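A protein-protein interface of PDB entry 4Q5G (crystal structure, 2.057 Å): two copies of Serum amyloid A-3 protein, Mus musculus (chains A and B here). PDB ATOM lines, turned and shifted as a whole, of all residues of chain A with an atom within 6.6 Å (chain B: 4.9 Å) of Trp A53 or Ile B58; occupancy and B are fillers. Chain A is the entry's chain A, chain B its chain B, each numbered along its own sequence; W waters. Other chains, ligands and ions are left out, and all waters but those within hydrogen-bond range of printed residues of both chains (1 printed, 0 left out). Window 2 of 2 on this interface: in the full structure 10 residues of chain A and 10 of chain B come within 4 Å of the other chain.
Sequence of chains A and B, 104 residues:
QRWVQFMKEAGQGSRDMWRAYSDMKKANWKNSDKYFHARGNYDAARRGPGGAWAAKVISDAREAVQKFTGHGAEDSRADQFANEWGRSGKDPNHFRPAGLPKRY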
ATOM      1  N   TRP A   3      11.008  13.662   8.719  1.00  0.00           N
ATOM      2  CA  TRP A   3      10.858  13.709  10.158  1.00  0.00           C
ATOM      3  C   TRP A   3      10.937  12.295  10.713  1.00  0.00           C
ATOM      4  O   TRP A   3      11.446  12.067  11.810  1.00  0.00           O
ATOM      5  CB  TRP A   3       9.523  14.371  10.516  1.00  0.00           C
ATOM      6  CG  TRP A   3       9.211  14.437  11.983  1.00  0.00           C
ATOM      7  CD1 TRP A   3       8.164  13.848  12.618  1.00  0.00           C
ATOM      8  CD2 TRP A   3       9.952  15.135  12.994  1.00  0.00           C
ATOM      9  NE1 TRP A   3       8.200  14.132  13.959  1.00  0.00           N
ATOM     10  CE2 TRP A   3       9.293  14.915  14.219  1.00  0.00           C
ATOM     11  CE3 TRP A   3      11.116  15.912  12.984  1.00  0.00           C
ATOM     12  CZ2 TRP A   3       9.743  15.451  15.415  1.00  0.00           C
ATOM     13  CZ3 TRP A   3      11.568  16.440  14.172  1.00  0.00           C
ATOM     14  CH2 TRP A   3      10.882  16.210  15.374  1.00  0.00           C
ATOM     15  N   PHE A   6      14.465  11.311  10.902  1.00  0.00           N
ATOM     16  CA  PHE A   6      15.042  12.020  12.039  1.00  0.00           C
ATOM     17  C   PHE A   6      14.747  11.302  13.357  1.00  0.00           C
ATOM     18  O   PHE A   6      15.653  11.075  14.158  1.00  0.00           O
ATOM     19  CB  PHE A   6      14.514  13.457  12.089  1.00  0.00           C
ATOM     20  CG  PHE A   6      15.153  14.308  13.135  1.00  0.00           C
ATOM     21  CD1 PHE A   6      16.325  14.994  12.865  1.00  0.00           C
ATOM     22  CD2 PHE A   6      14.578  14.439  14.393  1.00  0.00           C
ATOM     23  CE1 PHE A   6      16.916  15.792  13.830  1.00  0.00           C
ATOM     24  CE2 PHE A   6      15.162  15.230  15.363  1.00  0.00           C
ATOM     25  CZ  PHE A   6      16.336  15.910  15.083  1.00  0.00           C
ATOM     26  N   MET A   7      13.485  10.938  13.578  1.00  0.00           N
ATOM     27  CA  MET A   7      13.096  10.297  14.833  1.00  0.00           C
ATOM     28  C   MET A   7      13.740   8.915  14.935  1.00  0.00           C
ATOM     29  O   MET A   7      14.164   8.494  16.018  1.00  0.00           O
ATOM     30  CB  MET A   7      11.572  10.184  14.954  1.00  0.00           C
ATOM     31  CG  MET A   7      10.878  11.496  15.253  1.00  0.00           C
ATOM     32  SD  MET A   7      11.393  12.240  17.010  1.00  0.00           S
ATOM     33  CE  MET A   7      10.368  11.045  18.179  1.00  0.00           C
ATOM     34  N   ALA A  10      17.268   9.385  15.869  1.00  0.00           N
ATOM     35  CA  ALA A  10      17.277   9.820  17.262  1.00  0.00           C
ATOM     36  C   ALA A  10      17.100   8.626  18.197  1.00  0.00           C
ATOM     37  O   ALA A  10      17.717   8.571  19.264  1.00  0.00           O
ATOM     38  CB  ALA A  10      16.193  10.862  17.506  1.00  0.00           C
ATOM     39  N   SER A  14      19.948   7.362  20.760  1.00  0.00           N
ATOM     40  CA  SER A  14      19.627   7.220  22.175  1.00  0.00           C
ATOM     41  C   SER A  14      20.124   5.880  22.735  1.00  0.00           C
ATOM     42  O   SER A  14      20.628   5.825  23.861  1.00  0.00           O
ATOM     43  CB  SER A  14      18.120   7.366  22.403  1.00  0.00           C
ATOM     44  OG  SER A  14      17.704   8.682  22.068  1.00  0.00           O
ATOM     45  N   ALA A  44      26.429   7.945  18.399  1.00  0.00           N
ATOM     46  CA  ALA A  44      25.115   8.508  18.131  1.00  0.00           C
ATOM     47  C   ALA A  44      25.090   9.359  16.864  1.00  0.00           C
ATOM     48  O   ALA A  44      24.207   9.201  16.029  1.00  0.00           O
ATOM     49  CB  ALA A  44      24.648   9.319  19.327  1.00  0.00           C
ATOM     50  N   ALA A  45      26.079  10.235  16.711  1.00  0.00           N
ATOM     51  CA  ALA A  45      26.123  11.176  15.592  1.00  0.00           C
ATOM     52  C   ALA A  45      26.353  10.488  14.248  1.00  0.00           C
ATOM     53  O   ALA A  45      26.029  11.041  13.194  1.00  0.00           O
ATOM     54  CB  ALA A  45      27.206  12.228  15.830  1.00  0.00           C
ATOM     55  N   GLY A  48      23.319   9.762  11.994  1.00  0.00           N
ATOM     56  CA  GLY A  48      22.759  10.862  11.227  1.00  0.00           C
ATOM     57  C   GLY A  48      22.344  12.017  12.140  1.00  0.00           C
ATOM     58  O   GLY A  48      22.547  11.958  13.352  1.00  0.00           O
ATOM     59  N   PRO A  49      21.752  13.067  11.558  1.00  0.00           N
ATOM     60  CA  PRO A  49      21.304  14.274  12.268  1.00  0.00           C
ATOM     61  C   PRO A  49      20.417  13.994  13.490  1.00  0.00           C
ATOM     62  O   PRO A  49      20.647  14.584  14.545  1.00  0.00           O
ATOM     63  CB  PRO A  49      20.518  15.033  11.194  1.00  0.00           C
ATOM     64  CG  PRO A  49      21.087  14.554   9.906  1.00  0.00           C
ATOM     65  CD  PRO A  49      21.425  13.115  10.123  1.00  0.00           C
ATOM     66  N   GLY A  50      19.416  13.130  13.356  1.00  0.00           N
ATOM     67  CA  GLY A  50      18.614  12.727  14.504  1.00  0.00           C
ATOM     68  C   GLY A  50      19.470  12.121  15.611  1.00  0.00           C
ATOM     69  O   GLY A  50      19.195  12.301  16.802  1.00  0.00           O
ATOM     70  N   GLY A  51      20.527  11.415  15.220  1.00  0.00           N
ATOM     71  CA  GLY A  51      21.436  10.812  16.181  1.00  0.00           C
ATOM     72  C   GLY A  51      22.260  11.855  16.920  1.00  0.00           C
ATOM     73  O   GLY A  51      22.404  11.803  18.139  1.00  0.00           O
ATOM     74  N   ALA A  52      22.802  12.814  16.184  1.00  0.00           N
ATOM     75  CA  ALA A  52      23.542  13.904  16.806  1.00  0.00           C
ATOM     76  C   ALA A  52      22.645  14.771  17.695  1.00  0.00           C
ATOM     77  O   ALA A  52      23.065  15.201  18.771  1.00  0.00           O
ATOM     78  CB  ALA A  52      24.220  14.758  15.745  1.00  0.00           C
ATOM     79  N   TRP A  53      21.413  15.026  17.257  1.00  0.00           N
ATOM     80  CA  TRP A  53      20.480  15.786  18.081  1.00  0.00           C
ATOM     81  C   TRP A  53      20.221  15.045  19.389  1.00  0.00           C
ATOM     82  O   TRP A  53      20.321  15.623  20.470  1.00  0.00           O
ATOM     83  CB  TRP A  53      19.160  16.039  17.343  1.00  0.00           C
ATOM     84  CG  TRP A  53      18.113  16.611  18.251  1.00  0.00           C
ATOM     85  CD1 TRP A  53      17.956  17.920  18.600  1.00  0.00           C
ATOM     86  CD2 TRP A  53      17.094  15.885  18.935  1.00  0.00           C
ATOM     87  NE1 TRP A  53      16.894  18.056  19.461  1.00  0.00           N
ATOM     88  CE2 TRP A  53      16.352  16.817  19.690  1.00  0.00           C
ATOM     89  CE3 TRP A  53      16.730  14.535  18.983  1.00  0.00           C
ATOM     90  CZ2 TRP A  53      15.256  16.443  20.476  1.00  0.00           C
ATOM     91  CZ3 TRP A  53      15.652  14.162  19.769  1.00  0.00           C
ATOM     92  CH2 TRP A  53      14.927  15.113  20.505  1.00  0.00           C
ATOM     93  N   ALA A  54      19.918  13.756  19.298  1.00  0.00           N
ATOM     94  CA  ALA A  54      19.702  12.944  20.495  1.00  0.00           C
ATOM     95  C   ALA A  54      20.916  12.985  21.420  1.00  0.00           C
ATOM     96  O   ALA A  54      20.776  13.154  22.632  1.00  0.00           O
ATOM     97  CB  ALA A  54      19.379  11.494  20.116  1.00  0.00           C
ATOM     98  N   ALA A  55      22.110  12.820  20.866  1.00  0.00           N
ATOM     99  CA  ALA A  55      23.305  12.869  21.707  1.00  0.00           C
ATOM    100  C   ALA A  55      23.450  14.252  22.384  1.00  0.00           C
ATOM    101  O   ALA A  55      23.795  14.362  23.570  1.00  0.00           O
ATOM    102  CB  ALA A  55      24.540  12.541  20.886  1.00  0.00           C
ATOM    103  N   LYS A  56      23.188  15.312  21.637  1.00  0.00           N
ATOM    104  CA  LYS A  56      23.256  16.649  22.234  1.00  0.00           C
ATOM    105  C   LYS A  56      22.279  16.863  23.413  1.00  0.00           C
ATOM    106  O   LYS A  56      22.686  17.388  24.457  1.00  0.00           O
ATOM    107  CB  LYS A  56      23.010  17.730  21.183  1.00  0.00           C
ATOM    108  CG  LYS A  56      23.027  19.156  21.806  1.00  0.00           C
ATOM    109  CD  LYS A  56      22.758  20.220  20.769  1.00  0.00           C
ATOM    110  CE  LYS A  56      22.224  21.520  21.411  1.00  0.00           C
ATOM    111  NZ  LYS A  56      22.790  21.815  22.768  1.00  0.00           N
ATOM    112  N   VAL A  57      21.009  16.481  23.289  1.00  0.00           N
ATOM    113  CA  VAL A  57      20.083  16.787  24.387  1.00  0.00           C
ATOM    114  C   VAL A  57      20.313  15.844  25.582  1.00  0.00           C
ATOM    115  O   VAL A  57      20.173  16.247  26.728  1.00  0.00           O
ATOM    116  CB  VAL A  57      18.587  16.734  23.944  1.00  0.00           C
ATOM    117  CG1 VAL A  57      18.308  17.813  22.890  1.00  0.00           C
ATOM    118  CG2 VAL A  57      18.184  15.339  23.438  1.00  0.00           C
ATOM    119  N   ILE A  58      20.680  14.596  25.320  1.00  0.00           N
ATOM    120  CA  ILE A  58      20.972  13.673  26.409  1.00  0.00           C
ATOM    121  C   ILE A  58      22.223  14.136  27.160  1.00  0.00           C
ATOM    122  O   ILE A  58      22.276  14.070  28.388  1.00  0.00           O
ATOM    123  CB  ILE A  58      21.178  12.234  25.899  1.00  0.00           C
ATOM    124  CG1 ILE A  58      19.852  11.661  25.380  1.00  0.00           C
ATOM    125  CG2 ILE A  58      21.737  11.346  27.012  1.00  0.00           C
ATOM    126  CD1 ILE A  58      20.030  10.394  24.524  1.00  0.00           C
ATOM    127  N   ARG A  87      30.994  14.094  19.115  1.00  0.00           N
ATOM    128  CA  ARG A  87      29.851  14.396  18.270  1.00  0.00           C
ATOM    129  C   ARG A  87      30.314  14.973  16.941  1.00  0.00           C
ATOM    130  O   ARG A  87      29.635  14.830  15.922  1.00  0.00           O
ATOM    131  CB  ARG A  87      28.885  15.358  18.985  1.00  0.00           C
ATOM    132  CG  ARG A  87      27.432  15.213  18.578  1.00  0.00           C
ATOM    133  CD  ARG A  87      26.466  15.687  19.703  1.00  0.00           C
ATOM    134  NE  ARG A  87      26.653  17.071  20.075  1.00  0.00           N
ATOM    135  CZ  ARG A  87      26.879  17.503  21.310  1.00  0.00           C
ATOM    136  NH1 ARG A  87      26.932  16.657  22.335  1.00  0.00           N
ATOM    137  NH2 ARG A  87      27.041  18.795  21.511  1.00  0.00           N
ATOM    138  N   SER B  14       9.339   9.160  24.783  1.00  0.00           N
ATOM    139  CA  SER B  14       9.672   9.360  23.372  1.00  0.00           C
ATOM    140  C   SER B  14       8.823   8.462  22.466  1.00  0.00           C
ATOM    141  O   SER B  14       8.476   8.832  21.354  1.00  0.00           O
ATOM    142  CB  SER B  14      11.162   9.083  23.127  1.00  0.00           C
ATOM    143  OG  SER B  14      11.986   9.966  23.883  1.00  0.00           O
ATOM    144  N   MET B  17       5.445  10.227  22.245  1.00  0.00           N
ATOM    145  CA  MET B  17       5.470  11.369  21.348  1.00  0.00           C
ATOM    146  C   MET B  17       5.394  10.861  19.910  1.00  0.00           C
ATOM    147  O   MET B  17       4.724  11.446  19.064  1.00  0.00           O
ATOM    148  CB  MET B  17       6.735  12.203  21.561  1.00  0.00           C
ATOM    149  CG  MET B  17       6.818  12.877  22.904  1.00  0.00           C
ATOM    150  SD  MET B  17       5.484  14.311  23.049  1.00  0.00           S
ATOM    151  CE  MET B  17       6.337  15.680  21.912  1.00  0.00           C
ATOM    152  N   ALA B  54      11.594  14.316  27.997  1.00  0.00           N
ATOM    153  CA  ALA B  54      11.568  13.864  26.617  1.00  0.00           C
ATOM    154  C   ALA B  54      10.509  14.606  25.825  1.00  0.00           C
ATOM    155  O   ALA B  54      10.739  14.956  24.668  1.00  0.00           O
ATOM    156  CB  ALA B  54      11.321  12.349  26.544  1.00  0.00           C
ATOM    157  N   ALA B  55       9.331  14.812  26.414  1.00  0.00           N
ATOM    158  CA  ALA B  55       8.304  15.581  25.725  1.00  0.00           C
ATOM    159  C   ALA B  55       8.817  16.993  25.378  1.00  0.00           C
ATOM    160  O   ALA B  55       8.586  17.514  24.288  1.00  0.00           O
ATOM    161  CB  ALA B  55       7.049  15.680  26.577  1.00  0.00           C
ATOM    162  N   LYS B  56       9.494  17.624  26.324  1.00  0.00           N
ATOM    163  CA  LYS B  56       9.942  18.989  26.107  1.00  0.00           C
ATOM    164  C   LYS B  56      10.941  19.120  24.942  1.00  0.00           C
ATOM    165  O   LYS B  56      10.767  19.977  24.064  1.00  0.00           O
ATOM    166  CB  LYS B  56      10.551  19.556  27.386  1.00  0.00           C
ATOM    167  CG  LYS B  56      11.390  20.802  27.141  1.00  0.00           C
ATOM    168  CD  LYS B  56      12.118  21.244  28.410  1.00  0.00           C
ATOM    169  CE  LYS B  56      11.170  21.917  29.382  1.00  0.00           C
ATOM    170  NZ  LYS B  56      10.650  23.197  28.808  1.00  0.00           N
ATOM    171  N   VAL B  57      11.979  18.287  24.906  1.00  0.00           N
ATOM    172  CA  VAL B  57      13.022  18.465  23.872  1.00  0.00           C
ATOM    173  C   VAL B  57      12.514  18.013  22.488  1.00  0.00           C
ATOM    174  O   VAL B  57      12.849  18.610  21.450  1.00  0.00           O
ATOM    175  CB  VAL B  57      14.348  17.719  24.259  1.00  0.00           C
ATOM    176  CG1 VAL B  57      14.976  18.352  25.509  1.00  0.00           C
ATOM    177  CG2 VAL B  57      14.109  16.218  24.479  1.00  0.00           C
ATOM    178  N   ILE B  58      11.666  16.995  22.457  1.00  0.00           N
ATOM    179  CA  ILE B  58      11.112  16.552  21.176  1.00  0.00           C
ATOM    180  C   ILE B  58      10.147  17.600  20.633  1.00  0.00           C
ATOM    181  O   ILE B  58      10.144  17.892  19.433  1.00  0.00           O
ATOM    182  CB  ILE B  58      10.396  15.203  21.309  1.00  0.00           C
ATOM    183  CG1 ILE B  58      11.415  14.079  21.548  1.00  0.00           C
ATOM    184  CG2 ILE B  58       9.551  14.929  20.074  1.00  0.00           C
ATOM    185  CD1 ILE B  58      10.774  12.774  22.025  1.00  0.00           C
ATOM    186  N   SER B  59       9.344  18.177  21.525  1.00  0.00           N
ATOM    187  CA  SER B  59       8.489  19.301  21.158  1.00  0.00           C
ATOM    188  C   SER B  59       9.258  20.455  20.543  1.00  0.00           C
ATOM    189  O   SER B  59       8.835  21.004  19.531  1.00  0.00           O
ATOM    190  CB  SER B  59       7.710  19.820  22.373  1.00  0.00           C
ATOM    191  OG  SER B  59       6.637  18.952  22.692  1.00  0.00           O
ATOM    192  N   ASP B  60      10.380  20.833  21.155  1.00  0.00           N
ATOM    193  CA  ASP B  60      11.144  21.985  20.674  1.00  0.00           C
ATOM    194  C   ASP B  60      11.823  21.666  19.333  1.00  0.00           C
ATOM    195  O   ASP B  60      11.934  22.532  18.461  1.00  0.00           O
ATOM    196  CB  ASP B  60      12.169  22.429  21.727  1.00  0.00           C
ATOM    197  CG  ASP B  60      11.507  23.007  22.968  1.00  0.00           C
ATOM    198  OD1 ASP B  60      10.297  23.311  22.901  1.00  0.00           O
ATOM    199  OD2 ASP B  60      12.178  23.159  24.012  1.00  0.00           O
ATOM    200  N   ALA B  61      12.234  20.416  19.149  1.00  0.00           N
ATOM    201  CA  ALA B  61      12.834  19.996  17.875  1.00  0.00           C
ATOM    202  C   ALA B  61      11.818  20.035  16.749  1.00  0.00           C
ATOM    203  O   ALA B  61      12.113  20.489  15.639  1.00  0.00           O
ATOM    204  CB  ALA B  61      13.433  18.579  17.984  1.00  0.00           C
ATOM    205  N   ARG B  62      10.627  19.525  17.023  1.00  0.00           N
ATOM    206  CA  ARG B  62       9.557  19.553  16.038  1.00  0.00           C
ATOM    207  C   ARG B  62       9.226  20.996  15.624  1.00  0.00           C
ATOM    208  O   ARG B  62       9.046  21.285  14.435  1.00  0.00           O
ATOM    209  CB  ARG B  62       8.312  18.852  16.597  1.00  0.00           C
ATOM    210  CG  ARG B  62       7.083  18.960  15.729  1.00  0.00           C
ATOM    211  CD  ARG B  62       7.247  18.202  14.422  1.00  0.00           C
ATOM    212  NE  ARG B  62       6.012  18.214  13.642  1.00  0.00           N
ATOM    213  CZ  ARG B  62       5.878  17.664  12.438  1.00  0.00           C
ATOM    214  NH1 ARG B  62       6.905  17.050  11.870  1.00  0.00           N
ATOM    215  NH2 ARG B  62       4.715  17.729  11.807  1.00  0.00           N
HETATM  216  O   HOH W   1      15.360  19.753  21.397  1.00  0.00           O
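Hydrophobic or aromatic side chains of chain A within 4 Å of the printed part of chain B: Trp A3 and Trp A53.
Of the 11 printed residues of chain B, 4 touch a printed residue of chain A.
Hydrophobic or aromatic side chains of chain B that line the printed part of chain A: Ile B58 and Ala B61.
Along chain B the printed residues that touch a printed residue of chain A span positions 57 to 62.
Among the printed residues, pairs that only touch across the chains: Trp A3 with Arg B62 (3.5 Å), Trp A53 with Val B57 (3.4 Å), Trp A53 with Ile B58 (3.8 Å) and Trp A53 with Ala B61 (3.8 Å).
Water W1 bridges the backbone carbonyl oxygen of Val B57 (2.8 Å) and the indole nitrogen of Trp A53 (3.0 Å).
Of the printed residues of chain B, Trp A3 touches Arg B62 (3.5 Å).
Met A7 touches none of the printed residues of chain B.
Gly A51 touches none of the printed residues of chain B.
Of chain B, only Val B57, Ile B58 and Ala B61 come within 4 Å of Trp A53.
Of the printed residues of chain A, Val B57 touches Trp A53.
Of chain A, only Trp A53 (3.8 Å) comes within 4 Å of Ile B58.
Printed residues of chain A within 4 Å of Ala B61: Trp A53.
Of the printed residues of chain A, Arg B62 touches Trp A3 (3.5 Å).
The nearest printed residue of chain B that does not touch Trp A3 is Ala B61 (4.2 Å).
Positions printed for both chains: 14, 54, 55, 56, 57 and 58.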
